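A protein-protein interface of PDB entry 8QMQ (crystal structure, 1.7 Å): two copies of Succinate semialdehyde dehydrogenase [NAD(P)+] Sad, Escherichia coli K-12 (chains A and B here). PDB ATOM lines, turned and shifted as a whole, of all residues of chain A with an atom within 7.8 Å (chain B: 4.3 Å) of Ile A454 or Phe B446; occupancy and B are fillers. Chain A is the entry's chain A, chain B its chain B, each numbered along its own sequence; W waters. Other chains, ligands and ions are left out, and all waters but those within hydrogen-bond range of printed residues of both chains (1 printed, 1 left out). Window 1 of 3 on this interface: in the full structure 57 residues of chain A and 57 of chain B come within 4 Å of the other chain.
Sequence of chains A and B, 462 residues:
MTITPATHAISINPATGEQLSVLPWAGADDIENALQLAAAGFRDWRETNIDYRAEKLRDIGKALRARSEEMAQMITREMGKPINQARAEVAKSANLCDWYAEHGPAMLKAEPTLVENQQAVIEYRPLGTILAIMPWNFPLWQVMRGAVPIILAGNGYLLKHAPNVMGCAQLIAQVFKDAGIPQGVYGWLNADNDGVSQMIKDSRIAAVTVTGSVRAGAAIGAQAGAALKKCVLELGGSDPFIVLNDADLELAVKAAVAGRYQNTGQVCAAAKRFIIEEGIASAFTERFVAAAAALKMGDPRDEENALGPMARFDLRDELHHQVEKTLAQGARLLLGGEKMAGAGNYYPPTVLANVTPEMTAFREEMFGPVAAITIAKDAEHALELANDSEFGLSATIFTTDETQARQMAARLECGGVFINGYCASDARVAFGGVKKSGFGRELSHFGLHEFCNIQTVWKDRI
Of the printed residues of chain A, Phe B446 touches Ile A122 (3.8 Å) and Ile A454 (3.7 Å). Printed residues of chain A within 4 Å of Gly B415: Asn A453, Ile A454, Gln A455 and Thr A456. Of the printed residues of chain B, Glu A111 touches His B445 (2.7 Å). Of the printed residues of chain B, Thr A456 touches Gly B415 (2.9 Å) and Ala B430 (2.8 Å). Printed residues of chain B within 4 Å of Ile A122: Ala B430 (3.8 Å) and Phe B446 (3.8 Å). The nearest printed residue of chain A that does not touch Phe B446 is Glu A111 (4.01 Å). The nearest printed residue of chain B that does not touch Thr A456 is Phe B446 (6.2 Å).
Among the printed residues, merely in contact across the chains: Gln A455 with Gly B415 (3.2 Å), Asn A453 with Gly B415 (3.6 Å), Ile A454 with Gly B415 (3.6 Å), Ile A454 with Phe B446 (3.7 Å), Ile A122 with Ala B430 (3.8 Å), Ile A122 with Phe B446 (3.8 Å) and Ile A454 with Ala B430 (3.95 Å).
Water W1 lies within hydrogen-bond range of O of Cys A452 (2.9 Å), N of Ile A454 (3.1 Å) and NH2 of Arg B441 (3.4 Å).
The backbone NH of Glu A111 sits at hydrogen-bond distance from the backbone carbonyl oxygen of Ile A122 (2.9 Å). OH of Tyr A124 is in hydrogen-bond range of OE1 of Glu A111 (2.8 Å). N of Glu A123 is in hydrogen-bond range of O of Gln A455 (2.8 Å). The backbone carbonyl oxygen (O) of Arg A125 sits at hydrogen-bond distance from the backbone NH (N) of Asn A453, 2.7 Å away. The side-chain amide oxygen of Gln A455 lies within hydrogen-bond range of the guanidinium group of Arg A125, 2.7 Å away. The side-chain carboxylate (OE2) of Glu B450 sits at hydrogen-bond distance from the backbone NH (N) of Arg B441, 2.9 Å away.
Of the 11 printed residues of chain B, 5 touch a printed residue of chain A. Hydrophobic or aromatic side chains of chain B within 4 Å of the printed part of chain A: Ala B430, His B445 and Phe B446. Hydrophobic or aromatic side chains of chain A within 4 Å of the printed part of chain B: Ile A122 and Ile A454. Among the printed residues, 12 pairs touch across the chains. Among the printed residues, no Asp or Glu carboxylate lies within 4 Å of a Lys or Arg side-chain nitrogen of the other chain.
Positions printed for both chains: 449 and 450. Of the 12 pairs that touch across the chains among the printed residues, none has its exchanged pair printed and touching as well.
NE2 of His B445 lies within hydrogen-bond range of OE2 of Glu A111, at 2.7 Å. OD1 of Asn A453 is in hydrogen-bond range of NH2 of Arg B441 (2.8 Å). O of Ile A454 is in hydrogen-bond range of NE of Arg B441 (2.8 Å). The backbone carbonyl oxygen of Gly B415 is in hydrogen-bond range of the backbone NH of Thr A456 (2.9 Å). O of Ala B430 sits at hydrogen-bond distance from OG1 of Thr A456, 2.8 Å away.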
ATOM      1  N   GLU A 111      15.385 -22.842   2.642  1.00  0.00           N
ATOM      2  CA  GLU A 111      15.380 -24.228   3.049  1.00  0.00           C
ATOM      3  C   GLU A 111      16.549 -24.494   3.989  1.00  0.00           C
ATOM      4  O   GLU A 111      17.684 -24.111   3.673  1.00  0.00           O
ATOM      5  CB  GLU A 111      15.482 -25.092   1.793  1.00  0.00           C
ATOM      6  CG  GLU A 111      15.514 -26.568   1.955  1.00  0.00           C
ATOM      7  CD  GLU A 111      15.620 -27.239   0.600  1.00  0.00           C
ATOM      8  OE1 GLU A 111      14.692 -27.061  -0.226  1.00  0.00           O
ATOM      9  OE2 GLU A 111      16.644 -27.910   0.347  1.00  0.00           O
ATOM     10  N   PRO A 112      16.322 -25.115   5.144  1.00  0.00           N
ATOM     11  CA  PRO A 112      17.436 -25.422   6.045  1.00  0.00           C
ATOM     12  C   PRO A 112      18.321 -26.515   5.470  1.00  0.00           C
ATOM     13  O   PRO A 112      17.948 -27.228   4.534  1.00  0.00           O
ATOM     14  CB  PRO A 112      16.737 -25.894   7.325  1.00  0.00           C
ATOM     15  CG  PRO A 112      15.449 -26.459   6.848  1.00  0.00           C
ATOM     16  CD  PRO A 112      15.032 -25.588   5.680  1.00  0.00           C
ATOM     17  N   THR A 113      19.524 -26.625   6.036  1.00  0.00           N
ATOM     18  CA  THR A 113      20.472 -27.676   5.690  1.00  0.00           C
ATOM     19  C   THR A 113      20.951 -28.358   6.963  1.00  0.00           C
ATOM     20  O   THR A 113      20.665 -27.918   8.079  1.00  0.00           O
ATOM     21  CB  THR A 113      21.692 -27.136   4.916  1.00  0.00           C
ATOM     22  OG1 THR A 113      22.528 -26.389   5.808  1.00  0.00           O
ATOM     23  CG2 THR A 113      21.256 -26.243   3.758  1.00  0.00           C
ATOM     24  N   VAL A 121      21.680 -21.987   4.358  1.00  0.00           N
ATOM     25  CA  VAL A 121      20.354 -22.263   3.812  1.00  0.00           C
ATOM     26  C   VAL A 121      20.432 -22.309   2.290  1.00  0.00           C
ATOM     27  O   VAL A 121      21.404 -21.860   1.672  1.00  0.00           O
ATOM     28  CB  VAL A 121      19.305 -21.218   4.252  1.00  0.00           C
ATOM     29  CG1 VAL A 121      19.098 -21.258   5.766  1.00  0.00           C
ATOM     30  CG2 VAL A 121      19.725 -19.835   3.792  1.00  0.00           C
ATOM     31  N   ILE A 122      19.381 -22.858   1.685  1.00  0.00           N
ATOM     32  CA  ILE A 122      19.191 -22.840   0.240  1.00  0.00           C
ATOM     33  C   ILE A 122      18.111 -21.813  -0.074  1.00  0.00           C
ATOM     34  O   ILE A 122      17.014 -21.873   0.496  1.00  0.00           O
ATOM     35  CB  ILE A 122      18.781 -24.218  -0.309  1.00  0.00           C
ATOM     36  CG1 ILE A 122      19.719 -25.343   0.165  1.00  0.00           C
ATOM     37  CG2 ILE A 122      18.707 -24.159  -1.830  1.00  0.00           C
ATOM     38  CD1 ILE A 122      21.199 -25.126  -0.163  1.00  0.00           C
ATOM     39  N   GLU A 123      18.414 -20.879  -0.971  1.00  0.00           N
ATOM     40  CA  GLU A 123      17.461 -19.860  -1.397  1.00  0.00           C
ATOM     41  C   GLU A 123      17.058 -20.089  -2.851  1.00  0.00           C
ATOM     42  O   GLU A 123      17.830 -20.632  -3.646  1.00  0.00           O
ATOM     43  CB  GLU A 123      18.049 -18.450  -1.251  1.00  0.00           C
ATOM     44  CG  GLU A 123      18.443 -18.091   0.172  1.00  0.00           C
ATOM     45  CD  GLU A 123      17.314 -17.478   0.991  1.00  0.00           C
ATOM     46  OE1 GLU A 123      16.145 -17.440   0.523  1.00  0.00           O
ATOM     47  OE2 GLU A 123      17.611 -17.024   2.118  1.00  0.00           O
ATOM     48  N   TYR A 124      15.832 -19.683  -3.189  1.00  0.00           N
ATOM     49  CA  TYR A 124      15.277 -19.847  -4.535  1.00  0.00           C
ATOM     50  C   TYR A 124      15.168 -18.472  -5.182  1.00  0.00           C
ATOM     51  O   TYR A 124      14.210 -17.735  -4.934  1.00  0.00           O
ATOM     52  CB  TYR A 124      13.922 -20.566  -4.478  1.00  0.00           C
ATOM     53  CG  TYR A 124      14.086 -21.992  -4.017  1.00  0.00           C
ATOM     54  CD1 TYR A 124      14.323 -23.005  -4.934  1.00  0.00           C
ATOM     55  CD2 TYR A 124      14.072 -22.321  -2.661  1.00  0.00           C
ATOM     56  CE1 TYR A 124      14.512 -24.317  -4.529  1.00  0.00           C
ATOM     57  CE2 TYR A 124      14.265 -23.638  -2.240  1.00  0.00           C
ATOM     58  CZ  TYR A 124      14.479 -24.630  -3.186  1.00  0.00           C
ATOM     59  OH  TYR A 124      14.675 -25.943  -2.804  1.00  0.00           O
ATOM     60  N   ARG A 125      16.180 -18.119  -6.039  1.00  0.00           N
ATOM     61  CA  ARG A 125      16.247 -16.806  -6.666  1.00  0.00           C
ATOM     62  C   ARG A 125      15.707 -16.837  -8.090  1.00  0.00           C
ATOM     63  O   ARG A 125      15.778 -17.865  -8.767  1.00  0.00           O
ATOM     64  CB  ARG A 125      17.692 -16.305  -6.715  1.00  0.00           C
ATOM     65  CG  ARG A 125      18.464 -16.487  -5.430  1.00  0.00           C
ATOM     66  CD  ARG A 125      17.926 -15.629  -4.298  1.00  0.00           C
ATOM     67  NE  ARG A 125      18.943 -15.514  -3.255  1.00  0.00           N
ATOM     68  CZ  ARG A 125      18.731 -15.050  -2.032  1.00  0.00           C
ATOM     69  NH1 ARG A 125      17.533 -14.641  -1.641  1.00  0.00           N
ATOM     70  NH2 ARG A 125      19.752 -14.982  -1.181  1.00  0.00           N
ATOM     71  N   PRO A 126      15.178 -15.704  -8.558  1.00  0.00           N
ATOM     72  CA  PRO A 126      14.855 -15.562  -9.982  1.00  0.00           C
ATOM     73  C   PRO A 126      16.066 -15.801 -10.873  1.00  0.00           C
ATOM     74  O   PRO A 126      17.203 -15.466 -10.524  1.00  0.00           O
ATOM     75  CB  PRO A 126      14.385 -14.102 -10.095  1.00  0.00           C
ATOM     76  CG  PRO A 126      14.016 -13.689  -8.733  1.00  0.00           C
ATOM     77  CD  PRO A 126      14.852 -14.496  -7.784  1.00  0.00           C
ATOM     78  N   LEU A 127      15.804 -16.350 -12.058  1.00  0.00           N
ATOM     79  CA  LEU A 127      16.814 -16.595 -13.083  1.00  0.00           C
ATOM     80  C   LEU A 127      16.889 -15.487 -14.133  1.00  0.00           C
ATOM     81  O   LEU A 127      17.984 -15.058 -14.506  1.00  0.00           O
ATOM     82  CB  LEU A 127      16.523 -17.939 -13.756  1.00  0.00           C
ATOM     83  CG  LEU A 127      17.616 -18.736 -14.457  1.00  0.00           C
ATOM     84  CD1 LEU A 127      18.782 -19.057 -13.503  1.00  0.00           C
ATOM     85  CD2 LEU A 127      17.028 -20.028 -15.011  1.00  0.00           C
ATOM     86  N   LYS A 230      19.564 -23.321 -20.070  1.00  0.00           N
ATOM     87  CA  LYS A 230      18.769 -24.457 -19.628  1.00  0.00           C
ATOM     88  C   LYS A 230      17.456 -24.495 -20.396  1.00  0.00           C
ATOM     89  O   LYS A 230      16.871 -23.452 -20.703  1.00  0.00           O
ATOM     90  CB  LYS A 230      18.477 -24.357 -18.132  1.00  0.00           C
ATOM     91  CG  LYS A 230      17.686 -25.550 -17.596  1.00  0.00           C
ATOM     92  CD  LYS A 230      17.334 -25.408 -16.122  1.00  0.00           C
ATOM     93  CE  LYS A 230      16.325 -26.506 -15.744  1.00  0.00           C
ATOM     94  NZ  LYS A 230      16.046 -26.593 -14.288  1.00  0.00           N
ATOM     95  N   HIS A 449      10.411 -24.375  -9.422  1.00  0.00           N
ATOM     96  CA  HIS A 449      11.844 -24.422  -9.170  1.00  0.00           C
ATOM     97  C   HIS A 449      12.676 -24.604 -10.432  1.00  0.00           C
ATOM     98  O   HIS A 449      13.870 -24.286 -10.411  1.00  0.00           O
ATOM     99  CB  HIS A 449      12.167 -25.546  -8.180  1.00  0.00           C
ATOM    100  CG  HIS A 449      11.683 -25.283  -6.786  1.00  0.00           C
ATOM    101  ND1 HIS A 449      11.641 -26.262  -5.815  1.00  0.00           N
ATOM    102  CD2 HIS A 449      11.230 -24.150  -6.198  1.00  0.00           C
ATOM    103  CE1 HIS A 449      11.179 -25.744  -4.691  1.00  0.00           C
ATOM    104  NE2 HIS A 449      10.924 -24.464  -4.897  1.00  0.00           N
ATOM    105  N   GLU A 450      12.082 -25.087 -11.536  1.00  0.00           N
ATOM    106  CA  GLU A 450      12.886 -25.364 -12.725  1.00  0.00           C
ATOM    107  C   GLU A 450      13.598 -24.115 -13.231  1.00  0.00           C
ATOM    108  O   GLU A 450      14.713 -24.207 -13.756  1.00  0.00           O
ATOM    109  CB  GLU A 450      12.022 -25.954 -13.845  1.00  0.00           C
ATOM    110  CG  GLU A 450      11.664 -27.420 -13.665  1.00  0.00           C
ATOM    111  CD  GLU A 450      12.767 -28.384 -14.068  1.00  0.00           C
ATOM    112  OE1 GLU A 450      13.883 -27.940 -14.444  1.00  0.00           O
ATOM    113  OE2 GLU A 450      12.521 -29.607 -13.995  1.00  0.00           O
ATOM    114  N   PHE A 451      12.979 -22.945 -13.095  1.00  0.00           N
ATOM    115  CA  PHE A 451      13.587 -21.711 -13.567  1.00  0.00           C
ATOM    116  C   PHE A 451      13.952 -20.786 -12.409  1.00  0.00           C
ATOM    117  O   PHE A 451      13.884 -19.559 -12.530  1.00  0.00           O
ATOM    118  CB  PHE A 451      12.673 -21.039 -14.594  1.00  0.00           C
ATOM    119  CG  PHE A 451      12.455 -21.894 -15.813  1.00  0.00           C
ATOM    120  CD1 PHE A 451      13.497 -22.104 -16.709  1.00  0.00           C
ATOM    121  CD2 PHE A 451      11.251 -22.543 -16.023  1.00  0.00           C
ATOM    122  CE1 PHE A 451      13.325 -22.915 -17.817  1.00  0.00           C
ATOM    123  CE2 PHE A 451      11.067 -23.357 -17.130  1.00  0.00           C
ATOM    124  CZ  PHE A 451      12.097 -23.544 -18.029  1.00  0.00           C
ATOM    125  N   CYS A 452      14.363 -21.373 -11.286  1.00  0.00           N
ATOM    126  CA  CYS A 452      15.040 -20.646 -10.223  1.00  0.00           C
ATOM    127  C   CYS A 452      16.537 -20.896 -10.280  1.00  0.00           C
ATOM    128  O   CYS A 452      17.000 -21.946 -10.737  1.00  0.00           O
ATOM    129  CB  CYS A 452      14.541 -21.058  -8.841  1.00  0.00           C
ATOM    130  SG  CYS A 452      12.903 -20.447  -8.409  1.00  0.00           S
ATOM    131  N   ASN A 453      17.285 -19.902  -9.810  1.00  0.00           N
ATOM    132  CA  ASN A 453      18.675 -20.087  -9.419  1.00  0.00           C
ATOM    133  C   ASN A 453      18.664 -20.601  -7.987  1.00  0.00           C
ATOM    134  O   ASN A 453      18.351 -19.850  -7.060  1.00  0.00           O
ATOM    135  CB  ASN A 453      19.423 -18.764  -9.546  1.00  0.00           C
ATOM    136  CG  ASN A 453      20.738 -18.749  -8.791  1.00  0.00           C
ATOM    137  OD1 ASN A 453      21.322 -19.792  -8.472  1.00  0.00           O
ATOM    138  ND2 ASN A 453      21.208 -17.550  -8.497  1.00  0.00           N
ATOM    139  N   ILE A 454      18.957 -21.885  -7.810  1.00  0.00           N
ATOM    140  CA  ILE A 454      18.996 -22.485  -6.483  1.00  0.00           C
ATOM    141  C   ILE A 454      20.339 -22.103  -5.867  1.00  0.00           C
ATOM    142  O   ILE A 454      21.390 -22.526  -6.354  1.00  0.00           O
ATOM    143  CB  ILE A 454      18.811 -24.004  -6.555  1.00  0.00           C
ATOM    144  CG1 ILE A 454      17.354 -24.328  -6.931  1.00  0.00           C
ATOM    145  CG2 ILE A 454      19.232 -24.662  -5.247  1.00  0.00           C
ATOM    146  CD1 ILE A 454      17.085 -25.799  -7.275  1.00  0.00           C
ATOM    147  N   GLN A 455      20.310 -21.287  -4.807  1.00  0.00           N
ATOM    148  CA  GLN A 455      21.508 -20.605  -4.317  1.00  0.00           C
ATOM    149  C   GLN A 455      21.793 -20.975  -2.867  1.00  0.00           C
ATOM    150  O   GLN A 455      20.990 -20.678  -1.979  1.00  0.00           O
ATOM    151  CB  GLN A 455      21.342 -19.090  -4.446  1.00  0.00           C
ATOM    152  CG  GLN A 455      22.595 -18.250  -4.112  1.00  0.00           C
ATOM    153  CD  GLN A 455      22.223 -16.779  -3.964  1.00  0.00           C
ATOM    154  OE1 GLN A 455      21.444 -16.424  -3.082  1.00  0.00           O
ATOM    155  NE2 GLN A 455      22.743 -15.929  -4.851  1.00  0.00           N
ATOM    156  N   THR A 456      22.950 -21.592  -2.623  1.00  0.00           N
ATOM    157  CA  THR A 456      23.419 -21.795  -1.258  1.00  0.00           C
ATOM    158  C   THR A 456      23.883 -20.461  -0.680  1.00  0.00           C
ATOM    159  O   THR A 456      24.615 -19.726  -1.342  1.00  0.00           O
ATOM    160  CB  THR A 456      24.585 -22.786  -1.246  1.00  0.00           C
ATOM    161  OG1 THR A 456      24.125 -24.073  -1.672  1.00  0.00           O
ATOM    162  CG2 THR A 456      25.204 -22.890   0.155  1.00  0.00           C
ATOM    163  N   VAL A 457      23.463 -20.145   0.546  1.00  0.00           N
ATOM    164  CA  VAL A 457      23.984 -18.992   1.290  1.00  0.00           C
ATOM    165  C   VAL A 457      24.511 -19.504   2.628  1.00  0.00           C
ATOM    166  O   VAL A 457      23.758 -20.061   3.433  1.00  0.00           O
ATOM    167  CB  VAL A 457      22.926 -17.891   1.489  1.00  0.00           C
ATOM    168  CG1 VAL A 457      23.544 -16.690   2.224  1.00  0.00           C
ATOM    169  CG2 VAL A 457      22.354 -17.453   0.148  1.00  0.00           C
ATOM    170  N   GLY B 415      25.356 -19.160  -7.920  1.00  0.00           N
ATOM    171  CA  GLY B 415      24.686 -20.217  -7.189  1.00  0.00           C
ATOM    172  C   GLY B 415      25.131 -20.426  -5.762  1.00  0.00           C
ATOM    173  O   GLY B 415      24.545 -21.246  -5.055  1.00  0.00           O
ATOM    174  N   ALA B 430      23.791 -27.156  -1.968  1.00  0.00           N
ATOM    175  CA  ALA B 430      23.751 -27.181  -3.425  1.00  0.00           C
ATOM    176  C   ALA B 430      25.032 -26.587  -4.010  1.00  0.00           C
ATOM    177  O   ALA B 430      25.640 -25.677  -3.439  1.00  0.00           O
ATOM    178  CB  ALA B 430      22.533 -26.405  -3.947  1.00  0.00           C
ATOM    179  N   ARG B 441      22.090 -28.563 -10.667  1.00  0.00           N
ATOM    180  CA  ARG B 441      22.696 -28.477  -9.340  1.00  0.00           C
ATOM    181  C   ARG B 441      23.213 -29.832  -8.887  1.00  0.00           C
ATOM    182  O   ARG B 441      22.626 -30.870  -9.190  1.00  0.00           O
ATOM    183  CB  ARG B 441      21.702 -27.931  -8.306  1.00  0.00           C
ATOM    184  CG  ARG B 441      21.336 -26.460  -8.535  1.00  0.00           C
ATOM    185  CD  ARG B 441      22.521 -25.538  -8.214  1.00  0.00           C
ATOM    186  NE  ARG B 441      22.225 -24.125  -8.448  1.00  0.00           N
ATOM    187  CZ  ARG B 441      22.420 -23.497  -9.601  1.00  0.00           C
ATOM    188  NH1 ARG B 441      22.861 -24.137 -10.675  1.00  0.00           N
ATOM    189  NH2 ARG B 441      22.185 -22.189  -9.674  1.00  0.00           N
ATOM    190  N   LEU B 443      25.071 -32.228  -5.534  1.00  0.00           N
ATOM    191  CA  LEU B 443      25.189 -32.458  -4.093  1.00  0.00           C
ATOM    192  C   LEU B 443      23.857 -32.238  -3.373  1.00  0.00           C
ATOM    193  O   LEU B 443      22.846 -31.896  -4.003  1.00  0.00           O
ATOM    194  CB  LEU B 443      26.316 -31.597  -3.500  1.00  0.00           C
ATOM    195  CG  LEU B 443      27.719 -32.018  -3.970  1.00  0.00           C
ATOM    196  CD1 LEU B 443      28.811 -31.113  -3.406  1.00  0.00           C
ATOM    197  CD2 LEU B 443      27.989 -33.490  -3.616  1.00  0.00           C
ATOM    198  N   SER B 444      23.826 -32.511  -2.074  1.00  0.00           N
ATOM    199  CA  SER B 444      22.589 -32.590  -1.284  1.00  0.00           C
ATOM    200  C   SER B 444      21.555 -33.429  -2.052  1.00  0.00           C
ATOM    201  O   SER B 444      21.914 -34.372  -2.768  1.00  0.00           O
ATOM    202  CB  SER B 444      22.126 -31.196  -0.921  1.00  0.00           C
ATOM    203  OG  SER B 444      21.031 -31.251  -0.017  1.00  0.00           O
ATOM    204  N   HIS B 445      20.262 -33.098  -1.915  1.00  0.00           N
ATOM    205  CA  HIS B 445      19.235 -33.834  -2.652  1.00  0.00           C
ATOM    206  C   HIS B 445      19.211 -33.463  -4.133  1.00  0.00           C
ATOM    207  O   HIS B 445      18.671 -34.225  -4.947  1.00  0.00           O
ATOM    208  CB  HIS B 445      17.843 -33.620  -2.017  1.00  0.00           C
ATOM    209  CG  HIS B 445      17.442 -32.182  -1.845  1.00  0.00           C
ATOM    210  ND1 HIS B 445      16.794 -31.461  -2.829  1.00  0.00           N
ATOM    211  CD2 HIS B 445      17.558 -31.346  -0.786  1.00  0.00           C
ATOM    212  CE1 HIS B 445      16.548 -30.238  -2.390  1.00  0.00           C
ATOM    213  NE2 HIS B 445      17.009 -30.140  -1.154  1.00  0.00           N
ATOM    214  N   PHE B 446      19.807 -32.324  -4.503  1.00  0.00           N
ATOM    215  CA  PHE B 446      19.773 -31.876  -5.893  1.00  0.00           C
ATOM    216  C   PHE B 446      20.535 -32.836  -6.795  1.00  0.00           C
ATOM    217  O   PHE B 446      20.056 -33.203  -7.877  1.00  0.00           O
ATOM    218  CB  PHE B 446      20.351 -30.460  -5.991  1.00  0.00           C
ATOM    219  CG  PHE B 446      19.758 -29.511  -4.994  1.00  0.00           C
ATOM    220  CD1 PHE B 446      18.563 -28.861  -5.274  1.00  0.00           C
ATOM    221  CD2 PHE B 446      20.370 -29.289  -3.767  1.00  0.00           C
ATOM    222  CE1 PHE B 446      17.998 -27.992  -4.353  1.00  0.00           C
ATOM    223  CE2 PHE B 446      19.813 -28.426  -2.844  1.00  0.00           C
ATOM    224  CZ  PHE B 446      18.626 -27.775  -3.137  1.00  0.00           C
ATOM    225  N   GLY B 447      21.729 -33.255  -6.363  1.00  0.00           N
ATOM    226  CA  GLY B 447      22.504 -34.201  -7.145  1.00  0.00           C
ATOM    227  C   GLY B 447      21.858 -35.570  -7.250  1.00  0.00           C
ATOM    228  O   GLY B 447      22.133 -36.308  -8.199  1.00  0.00           O
ATOM    229  N   LEU B 448      21.016 -35.938  -6.275  1.00  0.00           N
ATOM    230  CA  LEU B 448      20.278 -37.198  -6.346  1.00  0.00           C
ATOM    231  C   LEU B 448      19.113 -37.114  -7.329  1.00  0.00           C
ATOM    232  O   LEU B 448      18.811 -38.089  -8.029  1.00  0.00           O
ATOM    233  CB  LEU B 448      19.732 -37.585  -4.967  1.00  0.00           C
ATOM    234  CG  LEU B 448      20.552 -38.276  -3.887  1.00  0.00           C
ATOM    235  CD1 LEU B 448      19.654 -38.500  -2.677  1.00  0.00           C
ATOM    236  CD2 LEU B 448      21.106 -39.607  -4.374  1.00  0.00           C
ATOM    237  N   HIS B 449      18.445 -35.961  -7.397  1.00  0.00           N
ATOM    238  CA  HIS B 449      17.212 -35.841  -8.169  1.00  0.00           C
ATOM    239  C   HIS B 449      17.421 -35.402  -9.617  1.00  0.00           C
ATOM    240  O   HIS B 449      16.513 -35.593 -10.436  1.00  0.00           O
ATOM    241  CB  HIS B 449      16.263 -34.850  -7.489  1.00  0.00           C
ATOM    242  CG  HIS B 449      15.733 -35.322  -6.173  1.00  0.00           C
ATOM    243  ND1 HIS B 449      15.155 -34.471  -5.255  1.00  0.00           N
ATOM    244  CD2 HIS B 449      15.688 -36.558  -5.621  1.00  0.00           C
ATOM    245  CE1 HIS B 449      14.785 -35.160  -4.190  1.00  0.00           C
ATOM    246  NE2 HIS B 449      15.088 -36.431  -4.390  1.00  0.00           N
ATOM    247  N   GLU B 450      18.575 -34.820  -9.959  1.00  0.00           N
ATOM    248  CA  GLU B 450      18.759 -34.287 -11.309  1.00  0.00           C
ATOM    249  C   GLU B 450      18.607 -35.371 -12.364  1.00  0.00           C
ATOM    250  O   GLU B 450      18.105 -35.114 -13.465  1.00  0.00           O
ATOM    251  CB  GLU B 450      20.136 -33.625 -11.451  1.00  0.00           C
ATOM    252  CG  GLU B 450      20.225 -32.229 -10.877  1.00  0.00           C
ATOM    253  CD  GLU B 450      19.626 -31.151 -11.773  1.00  0.00           C
ATOM    254  OE1 GLU B 450      19.159 -31.447 -12.901  1.00  0.00           O
ATOM    255  OE2 GLU B 450      19.627 -29.985 -11.337  1.00  0.00           O
HETATM  256  O   HOH W   1      19.190 -23.755 -10.226  1.00  0.00           O
